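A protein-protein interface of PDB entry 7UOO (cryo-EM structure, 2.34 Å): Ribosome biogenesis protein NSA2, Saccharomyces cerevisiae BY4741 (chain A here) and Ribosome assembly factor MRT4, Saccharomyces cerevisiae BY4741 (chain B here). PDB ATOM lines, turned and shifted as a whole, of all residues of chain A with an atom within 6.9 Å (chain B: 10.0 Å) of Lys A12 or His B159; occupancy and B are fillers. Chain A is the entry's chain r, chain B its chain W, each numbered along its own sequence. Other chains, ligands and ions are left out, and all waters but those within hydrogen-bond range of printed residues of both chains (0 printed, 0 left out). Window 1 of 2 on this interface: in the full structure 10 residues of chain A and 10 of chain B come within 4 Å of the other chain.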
ATOM      1  N   ASP A   5      -1.034  23.313 -13.011  1.00  0.00           N
ATOM      2  CA  ASP A   5       0.084  23.741 -13.857  1.00  0.00           C
ATOM      3  C   ASP A   5       1.170  22.663 -13.890  1.00  0.00           C
ATOM      4  O   ASP A   5       2.290  22.825 -13.392  1.00  0.00           O
ATOM      5  CB  ASP A   5       0.629  25.079 -13.375  1.00  0.00           C
ATOM      6  CG  ASP A   5       0.822  25.125 -11.872  1.00  0.00           C
ATOM      7  OD1 ASP A   5       0.453  24.145 -11.191  1.00  0.00           O
ATOM      8  OD2 ASP A   5       1.342  26.142 -11.369  1.00  0.00           O
ATOM      9  N   TYR A   6       0.822  21.546 -14.534  1.00  0.00           N
ATOM     10  CA  TYR A   6       1.680  20.366 -14.484  1.00  0.00           C
ATOM     11  C   TYR A   6       2.936  20.519 -15.335  1.00  0.00           C
ATOM     12  O   TYR A   6       3.975  19.951 -14.991  1.00  0.00           O
ATOM     13  CB  TYR A   6       0.894  19.120 -14.897  1.00  0.00           C
ATOM     14  CG  TYR A   6       0.106  19.251 -16.178  1.00  0.00           C
ATOM     15  CD1 TYR A   6       0.688  18.971 -17.407  1.00  0.00           C
ATOM     16  CD2 TYR A   6      -1.232  19.624 -16.157  1.00  0.00           C
ATOM     17  CE1 TYR A   6      -0.032  19.084 -18.579  1.00  0.00           C
ATOM     18  CE2 TYR A   6      -1.960  19.734 -17.321  1.00  0.00           C
ATOM     19  CZ  TYR A   6      -1.355  19.463 -18.529  1.00  0.00           C
ATOM     20  OH  TYR A   6      -2.080  19.576 -19.691  1.00  0.00           O
ATOM     21  N   ILE A   7       2.877  21.274 -16.432  1.00  0.00           N
ATOM     22  CA  ILE A   7       4.075  21.500 -17.239  1.00  0.00           C
ATOM     23  C   ILE A   7       5.086  22.337 -16.465  1.00  0.00           C
ATOM     24  O   ILE A   7       6.290  22.048 -16.476  1.00  0.00           O
ATOM     25  CB  ILE A   7       3.707  22.143 -18.590  1.00  0.00           C
ATOM     26  CG1 ILE A   7       3.050  21.114 -19.512  1.00  0.00           C
ATOM     27  CG2 ILE A   7       4.930  22.739 -19.268  1.00  0.00           C
ATOM     28  CD1 ILE A   7       3.950  19.957 -19.880  1.00  0.00           C
ATOM     29  N   GLU A   8       4.616  23.377 -15.774  1.00  0.00           N
ATOM     30  CA  GLU A   8       5.510  24.170 -14.936  1.00  0.00           C
ATOM     31  C   GLU A   8       6.066  23.351 -13.779  1.00  0.00           C
ATOM     32  O   GLU A   8       7.247  23.484 -13.436  1.00  0.00           O
ATOM     33  CB  GLU A   8       4.787  25.411 -14.423  1.00  0.00           C
ATOM     34  CG  GLU A   8       4.792  26.559 -15.410  1.00  0.00           C
ATOM     35  CD  GLU A   8       4.038  27.766 -14.902  1.00  0.00           C
ATOM     36  OE1 GLU A   8       3.912  27.916 -13.670  1.00  0.00           O
ATOM     37  OE2 GLU A   8       3.562  28.563 -15.740  1.00  0.00           O
ATOM     38  N   ARG A   9       5.241  22.496 -13.167  1.00  0.00           N
ATOM     39  CA  ARG A   9       5.758  21.621 -12.116  1.00  0.00           C
ATOM     40  C   ARG A   9       6.805  20.653 -12.663  1.00  0.00           C
ATOM     41  O   ARG A   9       7.808  20.372 -11.999  1.00  0.00           O
ATOM     42  CB  ARG A   9       4.617  20.858 -11.443  1.00  0.00           C
ATOM     43  CG  ARG A   9       3.651  21.743 -10.675  1.00  0.00           C
ATOM     44  CD  ARG A   9       2.880  20.967  -9.621  1.00  0.00           C
ATOM     45  NE  ARG A   9       2.179  19.811 -10.167  1.00  0.00           N
ATOM     46  CZ  ARG A   9       0.974  19.851 -10.719  1.00  0.00           C
ATOM     47  NH1 ARG A   9       0.310  20.988 -10.846  1.00  0.00           N
ATOM     48  NH2 ARG A   9       0.421  18.723 -11.153  1.00  0.00           N
ATOM     49  N   HIS A  10       6.590  20.138 -13.877  1.00  0.00           N
ATOM     50  CA  HIS A  10       7.567  19.248 -14.495  1.00  0.00           C
ATOM     51  C   HIS A  10       8.875  19.974 -14.782  1.00  0.00           C
ATOM     52  O   HIS A  10       9.958  19.402 -14.621  1.00  0.00           O
ATOM     53  CB  HIS A  10       6.994  18.653 -15.781  1.00  0.00           C
ATOM     54  CG  HIS A  10       7.939  17.734 -16.491  1.00  0.00           C
ATOM     55  ND1 HIS A  10       7.969  16.376 -16.263  1.00  0.00           N
ATOM     56  CD2 HIS A  10       8.891  17.980 -17.422  1.00  0.00           C
ATOM     57  CE1 HIS A  10       8.898  15.824 -17.024  1.00  0.00           C
ATOM     58  NE2 HIS A  10       9.473  16.776 -17.735  1.00  0.00           N
ATOM     59  N   ILE A  11       8.793  21.226 -15.235  1.00  0.00           N
ATOM     60  CA  ILE A  11       9.997  22.018 -15.468  1.00  0.00           C
ATOM     61  C   ILE A  11      10.721  22.279 -14.152  1.00  0.00           C
ATOM     62  O   ILE A  11      11.955  22.239 -14.083  1.00  0.00           O
ATOM     63  CB  ILE A  11       9.638  23.326 -16.197  1.00  0.00           C
ATOM     64  CG1 ILE A  11       9.188  23.035 -17.630  1.00  0.00           C
ATOM     65  CG2 ILE A  11      10.808  24.293 -16.200  1.00  0.00           C
ATOM     66  CD1 ILE A  11       8.718  24.260 -18.383  1.00  0.00           C
ATOM     67  N   LYS A  12       9.962  22.529 -13.085  1.00  0.00           N
ATOM     68  CA  LYS A  12      10.557  22.748 -11.771  1.00  0.00           C
ATOM     69  C   LYS A  12      11.218  21.487 -11.226  1.00  0.00           C
ATOM     70  O   LYS A  12      12.223  21.578 -10.514  1.00  0.00           O
ATOM     71  CB  LYS A  12       9.485  23.246 -10.803  1.00  0.00           C
ATOM     72  CG  LYS A  12       9.888  24.454  -9.987  1.00  0.00           C
ATOM     73  CD  LYS A  12       8.691  25.038  -9.261  1.00  0.00           C
ATOM     74  CE  LYS A  12       7.633  25.514 -10.243  1.00  0.00           C
ATOM     75  NZ  LYS A  12       6.403  25.977  -9.551  1.00  0.00           N
ATOM     76  N   GLN A  13      10.674  20.311 -11.541  1.00  0.00           N
ATOM     77  CA  GLN A  13      11.172  19.068 -10.962  1.00  0.00           C
ATOM     78  C   GLN A  13      12.270  18.402 -11.782  1.00  0.00           C
ATOM     79  O   GLN A  13      13.147  17.753 -11.202  1.00  0.00           O
ATOM     80  CB  GLN A  13      10.021  18.076 -10.773  1.00  0.00           C
ATOM     81  CG  GLN A  13       9.054  18.437  -9.661  1.00  0.00           C
ATOM     82  CD  GLN A  13       9.668  18.307  -8.283  1.00  0.00           C
ATOM     83  OE1 GLN A  13       9.683  17.225  -7.698  1.00  0.00           O
ATOM     84  NE2 GLN A  13      10.178  19.414  -7.752  1.00  0.00           N
ATOM     85  N   HIS A  14      12.243  18.529 -13.109  1.00  0.00           N
ATOM     86  CA  HIS A  14      13.194  17.846 -13.973  1.00  0.00           C
ATOM     87  C   HIS A  14      13.998  18.774 -14.871  1.00  0.00           C
ATOM     88  O   HIS A  14      14.912  18.300 -15.552  1.00  0.00           O
ATOM     89  CB  HIS A  14      12.472  16.821 -14.864  1.00  0.00           C
ATOM     90  CG  HIS A  14      11.557  15.903 -14.117  1.00  0.00           C
ATOM     91  ND1 HIS A  14      11.994  14.746 -13.512  1.00  0.00           N
ATOM     92  CD2 HIS A  14      10.225  15.969 -13.883  1.00  0.00           C
ATOM     93  CE1 HIS A  14      10.973  14.141 -12.933  1.00  0.00           C
ATOM     94  NE2 HIS A  14       9.887  14.863 -13.144  1.00  0.00           N
ATOM     95  N   GLY A  15      13.691  20.063 -14.901  1.00  0.00           N
ATOM     96  CA  GLY A  15      14.357  20.963 -15.814  1.00  0.00           C
ATOM     97  C   GLY A  15      13.859  20.801 -17.239  1.00  0.00           C
ATOM     98  O   GLY A  15      12.840  20.163 -17.516  1.00  0.00           O
ATOM     99  N   ILE B 141      23.188  15.905  -2.941  1.00  0.00           N
ATOM    100  CA  ILE B 141      22.506  17.170  -3.171  1.00  0.00           C
ATOM    101  C   ILE B 141      23.486  18.317  -2.966  1.00  0.00           C
ATOM    102  O   ILE B 141      24.206  18.367  -1.961  1.00  0.00           O
ATOM    103  CB  ILE B 141      21.291  17.299  -2.241  1.00  0.00           C
ATOM    104  CG1 ILE B 141      20.317  16.144  -2.483  1.00  0.00           C
ATOM    105  CG2 ILE B 141      20.596  18.636  -2.445  1.00  0.00           C
ATOM    106  CD1 ILE B 141      19.132  16.141  -1.550  1.00  0.00           C
ATOM    107  N   VAL B 142      23.529  19.232  -3.925  1.00  0.00           N
ATOM    108  CA  VAL B 142      24.400  20.398  -3.847  1.00  0.00           C
ATOM    109  C   VAL B 142      23.663  21.494  -3.089  1.00  0.00           C
ATOM    110  O   VAL B 142      22.545  21.871  -3.455  1.00  0.00           O
ATOM    111  CB  VAL B 142      24.822  20.873  -5.243  1.00  0.00           C
ATOM    112  CG1 VAL B 142      25.582  22.182  -5.150  1.00  0.00           C
ATOM    113  CG2 VAL B 142      25.671  19.812  -5.921  1.00  0.00           C
ATOM    114  N   TYR B 143      24.284  21.996  -2.030  1.00  0.00           N
ATOM    115  CA  TYR B 143      23.692  23.022  -1.188  1.00  0.00           C
ATOM    116  C   TYR B 143      24.274  24.387  -1.534  1.00  0.00           C
ATOM    117  O   TYR B 143      25.266  24.502  -2.257  1.00  0.00           O
ATOM    118  CB  TYR B 143      23.907  22.681   0.289  1.00  0.00           C
ATOM    119  CG  TYR B 143      23.120  21.474   0.740  1.00  0.00           C
ATOM    120  CD1 TYR B 143      23.606  20.190   0.541  1.00  0.00           C
ATOM    121  CD2 TYR B 143      21.886  21.618   1.354  1.00  0.00           C
ATOM    122  CE1 TYR B 143      22.885  19.082   0.943  1.00  0.00           C
ATOM    123  CE2 TYR B 143      21.160  20.518   1.762  1.00  0.00           C
ATOM    124  CZ  TYR B 143      21.664  19.253   1.555  1.00  0.00           C
ATOM    125  OH  TYR B 143      20.942  18.156   1.960  1.00  0.00           O
ATOM    126  N   SER B 144      23.626  25.435  -1.015  1.00  0.00           N
ATOM    127  CA  SER B 144      23.982  26.797  -1.406  1.00  0.00           C
ATOM    128  C   SER B 144      25.390  27.166  -0.951  1.00  0.00           C
ATOM    129  O   SER B 144      26.122  27.843  -1.680  1.00  0.00           O
ATOM    130  CB  SER B 144      22.958  27.790  -0.856  1.00  0.00           C
ATOM    131  OG  SER B 144      22.912  27.766   0.557  1.00  0.00           O
ATOM    132  N   VAL B 155      20.336  25.866   3.150  1.00  0.00           N
ATOM    133  CA  VAL B 155      19.242  25.724   2.182  1.00  0.00           C
ATOM    134  C   VAL B 155      19.787  25.095   0.906  1.00  0.00           C
ATOM    135  O   VAL B 155      20.870  25.495   0.443  1.00  0.00           O
ATOM    136  CB  VAL B 155      18.608  27.091   1.901  1.00  0.00           C
ATOM    137  CG1 VAL B 155      17.625  27.014   0.744  1.00  0.00           C
ATOM    138  CG2 VAL B 155      17.920  27.623   3.151  1.00  0.00           C
ATOM    139  N   PRO B 156      19.105  24.109   0.318  1.00  0.00           N
ATOM    140  CA  PRO B 156      19.597  23.513  -0.930  1.00  0.00           C
ATOM    141  C   PRO B 156      19.645  24.530  -2.061  1.00  0.00           C
ATOM    142  O   PRO B 156      18.880  25.497  -2.092  1.00  0.00           O
ATOM    143  CB  PRO B 156      18.578  22.405  -1.220  1.00  0.00           C
ATOM    144  CG  PRO B 156      17.982  22.087   0.102  1.00  0.00           C
ATOM    145  CD  PRO B 156      17.939  23.385   0.851  1.00  0.00           C
ATOM    146  N   MET B 157      20.580  24.308  -2.983  1.00  0.00           N
ATOM    147  CA  MET B 157      20.758  25.208  -4.115  1.00  0.00           C
ATOM    148  C   MET B 157      19.498  25.250  -4.970  1.00  0.00           C
ATOM    149  O   MET B 157      18.871  24.221  -5.236  1.00  0.00           O
ATOM    150  CB  MET B 157      21.955  24.760  -4.956  1.00  0.00           C
ATOM    151  CG  MET B 157      22.268  25.664  -6.137  1.00  0.00           C
ATOM    152  SD  MET B 157      23.249  27.106  -5.686  1.00  0.00           S
ATOM    153  CE  MET B 157      24.889  26.390  -5.616  1.00  0.00           C
ATOM    154  N   ILE B 158      19.119  26.459  -5.390  1.00  0.00           N
ATOM    155  CA  ILE B 158      17.905  26.633  -6.176  1.00  0.00           C
ATOM    156  C   ILE B 158      18.084  25.985  -7.544  1.00  0.00           C
ATOM    157  O   ILE B 158      19.185  25.971  -8.112  1.00  0.00           O
ATOM    158  CB  ILE B 158      17.544  28.127  -6.280  1.00  0.00           C
ATOM    159  CG1 ILE B 158      16.143  28.309  -6.868  1.00  0.00           C
ATOM    160  CG2 ILE B 158      18.579  28.891  -7.085  1.00  0.00           C
ATOM    161  CD1 ILE B 158      15.053  27.652  -6.052  1.00  0.00           C
ATOM    162  N   HIS B 159      17.000  25.401  -8.062  1.00  0.00           N
ATOM    163  CA  HIS B 159      17.060  24.647  -9.308  1.00  0.00           C
ATOM    164  C   HIS B 159      17.346  25.524 -10.519  1.00  0.00           C
ATOM    165  O   HIS B 159      17.799  25.009 -11.545  1.00  0.00           O
ATOM    166  CB  HIS B 159      15.747  23.895  -9.517  1.00  0.00           C
ATOM    167  CG  HIS B 159      14.547  24.788  -9.559  1.00  0.00           C
ATOM    168  ND1 HIS B 159      13.921  25.246  -8.420  1.00  0.00           N
ATOM    169  CD2 HIS B 159      13.866  25.318 -10.602  1.00  0.00           C
ATOM    170  CE1 HIS B 159      12.901  26.014  -8.760  1.00  0.00           C
ATOM    171  NE2 HIS B 159      12.848  26.076 -10.078  1.00  0.00           N
ATOM    172  N   SER B 160      17.094  26.832 -10.423  1.00  0.00           N
ATOM    173  CA  SER B 160      17.288  27.724 -11.561  1.00  0.00           C
ATOM    174  C   SER B 160      18.754  27.897 -11.933  1.00  0.00           C
ATOM    175  O   SER B 160      19.048  28.274 -13.072  1.00  0.00           O
ATOM    176  CB  SER B 160      16.668  29.089 -11.267  1.00  0.00           C
ATOM    177  OG  SER B 160      15.311  28.959 -10.885  1.00  0.00           O
ATOM    178  N   LEU B 161      19.676  27.639 -11.010  1.00  0.00           N
ATOM    179  CA  LEU B 161      21.099  27.800 -11.271  1.00  0.00           C
ATOM    180  C   LEU B 161      21.733  26.572 -11.911  1.00  0.00           C
ATOM    181  O   LEU B 161      22.926  26.607 -12.227  1.00  0.00           O
ATOM    182  CB  LEU B 161      21.837  28.137  -9.970  1.00  0.00           C
ATOM    183  CG  LEU B 161      21.505  29.496  -9.354  1.00  0.00           C
ATOM    184  CD1 LEU B 161      22.199  29.665  -8.017  1.00  0.00           C
ATOM    185  CD2 LEU B 161      21.891  30.620 -10.304  1.00  0.00           C
ATOM    186  N   GLU B 162      20.970  25.496 -12.100  1.00  0.00           N
ATOM    187  CA  GLU B 162      21.532  24.282 -12.685  1.00  0.00           C
ATOM    188  C   GLU B 162      22.074  24.468 -14.102  1.00  0.00           C
ATOM    189  O   GLU B 162      23.162  23.933 -14.379  1.00  0.00           O
ATOM    190  CB  GLU B 162      20.493  23.153 -12.629  1.00  0.00           C
ATOM    191  CG  GLU B 162      21.087  21.754 -12.677  1.00  0.00           C
ATOM    192  CD  GLU B 162      21.318  21.260 -14.090  1.00  0.00           C
ATOM    193  OE1 GLU B 162      20.742  21.844 -15.029  1.00  0.00           O
ATOM    194  OE2 GLU B 162      22.079  20.284 -14.263  1.00  0.00           O
ATOM    195  N   PRO B 163      21.394  25.149 -15.040  1.00  0.00           N
ATOM    196  CA  PRO B 163      22.045  25.397 -16.340  1.00  0.00           C
ATOM    197  C   PRO B 163      23.323  26.211 -16.232  1.00  0.00           C
ATOM    198  O   PRO B 163      24.273  25.966 -16.985  1.00  0.00           O
ATOM    199  CB  PRO B 163      20.965  26.137 -17.140  1.00  0.00           C
ATOM    200  CG  PRO B 163      19.694  25.716 -16.527  1.00  0.00           C
ATOM    201  CD  PRO B 163      19.986  25.594 -15.067  1.00  0.00           C
ATOM    202  N   THR B 164      23.369  27.174 -15.307  1.00  0.00           N
ATOM    203  CA  THR B 164      24.586  27.954 -15.102  1.00  0.00           C
ATOM    204  C   THR B 164      25.729  27.073 -14.614  1.00  0.00           C
ATOM    205  O   THR B 164      26.863  27.192 -15.092  1.00  0.00           O
ATOM    206  CB  THR B 164      24.321  29.086 -14.107  1.00  0.00           C
ATOM    207  OG1 THR B 164      23.289  29.939 -14.615  1.00  0.00           O
ATOM    208  CG2 THR B 164      25.581  29.909 -13.879  1.00  0.00           C
ATOM    209  N   MET B 165      25.443  26.172 -13.672  1.00  0.00           N
ATOM    210  CA  MET B 165      26.481  25.284 -13.158  1.00  0.00           C
ATOM    211  C   MET B 165      26.927  24.280 -14.212  1.00  0.00           C
ATOM    212  O   MET B 165      28.110  23.927 -14.278  1.00  0.00           O
ATOM    213  CB  MET B 165      25.982  24.563 -11.909  1.00  0.00           C
ATOM    214  CG  MET B 165      25.682  25.484 -10.741  1.00  0.00           C
ATOM    215  SD  MET B 165      25.212  24.577  -9.257  1.00  0.00           S
ATOM    216  CE  MET B 165      26.674  23.577  -8.997  1.00  0.00           C
ATOM    217  N   ARG B 166      25.997  23.800 -15.040  1.00  0.00           N
ATOM    218  CA  ARG B 166      26.353  22.791 -16.032  1.00  0.00           C
ATOM    219  C   ARG B 166      27.123  23.388 -17.206  1.00  0.00           C
ATOM    220  O   ARG B 166      28.088  22.785 -17.687  1.00  0.00           O
ATOM    221  CB  ARG B 166      25.101  22.070 -16.529  1.00  0.00           C
ATOM    222  CG  ARG B 166      25.406  20.828 -17.352  1.00  0.00           C
ATOM    223  CD  ARG B 166      24.147  20.121 -17.824  1.00  0.00           C
ATOM    224  NE  ARG B 166      23.341  20.954 -18.708  1.00  0.00           N
ATOM    225  CZ  ARG B 166      22.142  21.428 -18.400  1.00  0.00           C
ATOM    226  NH1 ARG B 166      21.568  21.152 -17.242  1.00  0.00           N
ATOM    227  NH2 ARG B 166      21.501  22.193 -19.278  1.00  0.00           N
ATOM    228  N   THR B 173      26.115  18.222 -13.498  1.00  0.00           N
ATOM    229  CA  THR B 173      25.014  18.237 -12.547  1.00  0.00           C
ATOM    230  C   THR B 173      23.773  17.605 -13.160  1.00  0.00           C
ATOM    231  O   THR B 173      23.599  17.587 -14.382  1.00  0.00           O
ATOM    232  CB  THR B 173      24.675  19.665 -12.091  1.00  0.00           C
ATOM    233  OG1 THR B 173      24.228  20.435 -13.212  1.00  0.00           O
ATOM    234  CG2 THR B 173      25.890  20.335 -11.475  1.00  0.00           C
ATOM    235  N   LYS B 174      22.912  17.084 -12.292  1.00  0.00           N
ATOM    236  CA  LYS B 174      21.624  16.533 -12.679  1.00  0.00           C
ATOM    237  C   LYS B 174      20.552  17.125 -11.779  1.00  0.00           C
ATOM    238  O   LYS B 174      20.842  17.693 -10.724  1.00  0.00           O
ATOM    239  CB  LYS B 174      21.593  14.999 -12.583  1.00  0.00           C
ATOM    240  CG  LYS B 174      22.331  14.266 -13.693  1.00  0.00           C
ATOM    241  CD  LYS B 174      23.813  14.120 -13.393  1.00  0.00           C
ATOM    242  CE  LYS B 174      24.537  13.416 -14.529  1.00  0.00           C
ATOM    243  NZ  LYS B 174      26.013  13.440 -14.349  1.00  0.00           N
ATOM    244  N   ILE B 175      19.303  16.995 -12.209  1.00  0.00           N
ATOM    245  CA  ILE B 175      18.157  17.470 -11.446  1.00  0.00           C
ATOM    246  C   ILE B 175      17.361  16.250 -11.010  1.00  0.00           C
ATOM    247  O   ILE B 175      16.795  15.534 -11.844  1.00  0.00           O
ATOM    248  CB  ILE B 175      17.291  18.438 -12.262  1.00  0.00           C
ATOM    249  CG1 ILE B 175      18.153  19.568 -12.823  1.00  0.00           C
ATOM    250  CG2 ILE B 175      16.176  19.005 -11.406  1.00  0.00           C
ATOM    251  CD1 ILE B 175      17.402  20.519 -13.715  1.00  0.00           C
ATOM    252  N   LYS B 176      17.325  16.003  -9.702  1.00  0.00           N
ATOM    253  CA  LYS B 176      16.517  14.938  -9.116  1.00  0.00           C
ATOM    254  C   LYS B 176      15.487  15.583  -8.200  1.00  0.00           C
ATOM    255  O   LYS B 176      15.850  16.197  -7.190  1.00  0.00           O
ATOM    256  CB  LYS B 176      17.379  13.937  -8.347  1.00  0.00           C
ATOM    257  CG  LYS B 176      18.310  13.095  -9.205  1.00  0.00           C
ATOM    258  CD  LYS B 176      18.874  11.931  -8.397  1.00  0.00           C
ATOM    259  CE  LYS B 176      19.845  11.087  -9.208  1.00  0.00           C
ATOM    260  NZ  LYS B 176      21.158  11.766  -9.405  1.00  0.00           N
ATOM    261  N   ALA B 177      14.208  15.446  -8.566  1.00  0.00           N
ATOM    262  CA  ALA B 177      13.079  15.959  -7.783  1.00  0.00           C
ATOM    263  C   ALA B 177      13.242  17.444  -7.469  1.00  0.00           C
ATOM    264  O   ALA B 177      12.950  17.906  -6.365  1.00  0.00           O
ATOM    265  CB  ALA B 177      12.882  15.147  -6.502  1.00  0.00           C
ATOM    266  N   GLY B 178      13.723  18.198  -8.453  1.00  0.00           N
ATOM    267  CA  GLY B 178      13.912  19.621  -8.273  1.00  0.00           C
ATOM    268  C   GLY B 178      15.141  20.015  -7.491  1.00  0.00           C
ATOM    269  O   GLY B 178      15.223  21.156  -7.030  1.00  0.00           O
ATOM    270  N   LYS B 179      16.103  19.110  -7.321  1.00  0.00           N
ATOM    271  CA  LYS B 179      17.319  19.401  -6.578  1.00  0.00           C
ATOM    272  C   LYS B 179      18.543  19.110  -7.431  1.00  0.00           C
ATOM    273  O   LYS B 179      18.570  18.132  -8.184  1.00  0.00           O
ATOM    274  CB  LYS B 179      17.377  18.593  -5.279  1.00  0.00           C
ATOM    275  CG  LYS B 179      16.302  18.983  -4.283  1.00  0.00           C
ATOM    276  CD  LYS B 179      16.478  18.273  -2.959  1.00  0.00           C
ATOM    277  CE  LYS B 179      15.530  18.830  -1.914  1.00  0.00           C
ATOM    278  NZ  LYS B 179      15.760  18.234  -0.572  1.00  0.00           N
ATOM    279  N   ILE B 180      19.552  19.966  -7.307  1.00  0.00           N
ATOM    280  CA  ILE B 180      20.798  19.803  -8.048  1.00  0.00           C
ATOM    281  C   ILE B 180      21.649  18.746  -7.357  1.00  0.00           C
ATOM    282  O   ILE B 180      21.880  18.810  -6.145  1.00  0.00           O
ATOM    283  CB  ILE B 180      21.542  21.142  -8.156  1.00  0.00           C
ATOM    284  CG1 ILE B 180      20.625  22.199  -8.776  1.00  0.00           C
ATOM    285  CG2 ILE B 180      22.810  20.983  -8.975  1.00  0.00           C
ATOM    286  CD1 ILE B 180      21.279  23.539  -8.974  1.00  0.00           C
ATOM    287  N   THR B 181      22.110  17.764  -8.128  1.00  0.00           N
ATOM    288  CA  THR B 181      22.823  16.614  -7.594  1.00  0.00           C
ATOM    289  C   THR B 181      24.041  16.327  -8.462  1.00  0.00           C
ATOM    290  O   THR B 181      24.032  16.578  -9.669  1.00  0.00           O
ATOM    291  CB  THR B 181      21.904  15.379  -7.538  1.00  0.00           C
ATOM    292  OG1 THR B 181      20.607  15.769  -7.068  1.00  0.00           O
ATOM    293  CG2 THR B 181      22.461  14.319  -6.604  1.00  0.00           C
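Lys A12 touches His B159.
Lys A12 touches Gly B178.
Ile B175 touches Gln A13 (CG2 to O, 3.3 Å).
Ile B175 touches His A14.
Gly A15 touches Ile B175 (CA to CD1, 3.7 Å).
The side-chain amide nitrogen (NE2) of Gln A13 is in hydrogen-bond range of the backbone carbonyl oxygen (O) of Ala B177.
The backbone carbonyl oxygen of Gln A13 lies within hydrogen-bond range of the backbone NH of Gly B178 (2.8 Å).
Of chain B, only His B159 (3.4 Å) and Gly B178 (3.4 Å) come within 4 Å of Lys A12.
Gln A13 touches just these residues of chain B: Ile B175, Ala B177 and Gly B178.
Of the printed residues of chain A, Ile B175 touches Gln A13, His A14 and Gly A15.
Printed residues of chain A within 4 Å of Gly B178: Lys A12 and Gln A13.
The nearest residue of chain B that does not touch Lys A12 is Ile B175 (4.8 Å).
The nearest printed residue of chain B that does not touch His A14 is Gly B178 (4.9 Å).
Along chain B the printed residues that touch a printed residue of chain A span positions 159 to 178.
Among the printed residues, 7 pairs touch across the chains.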
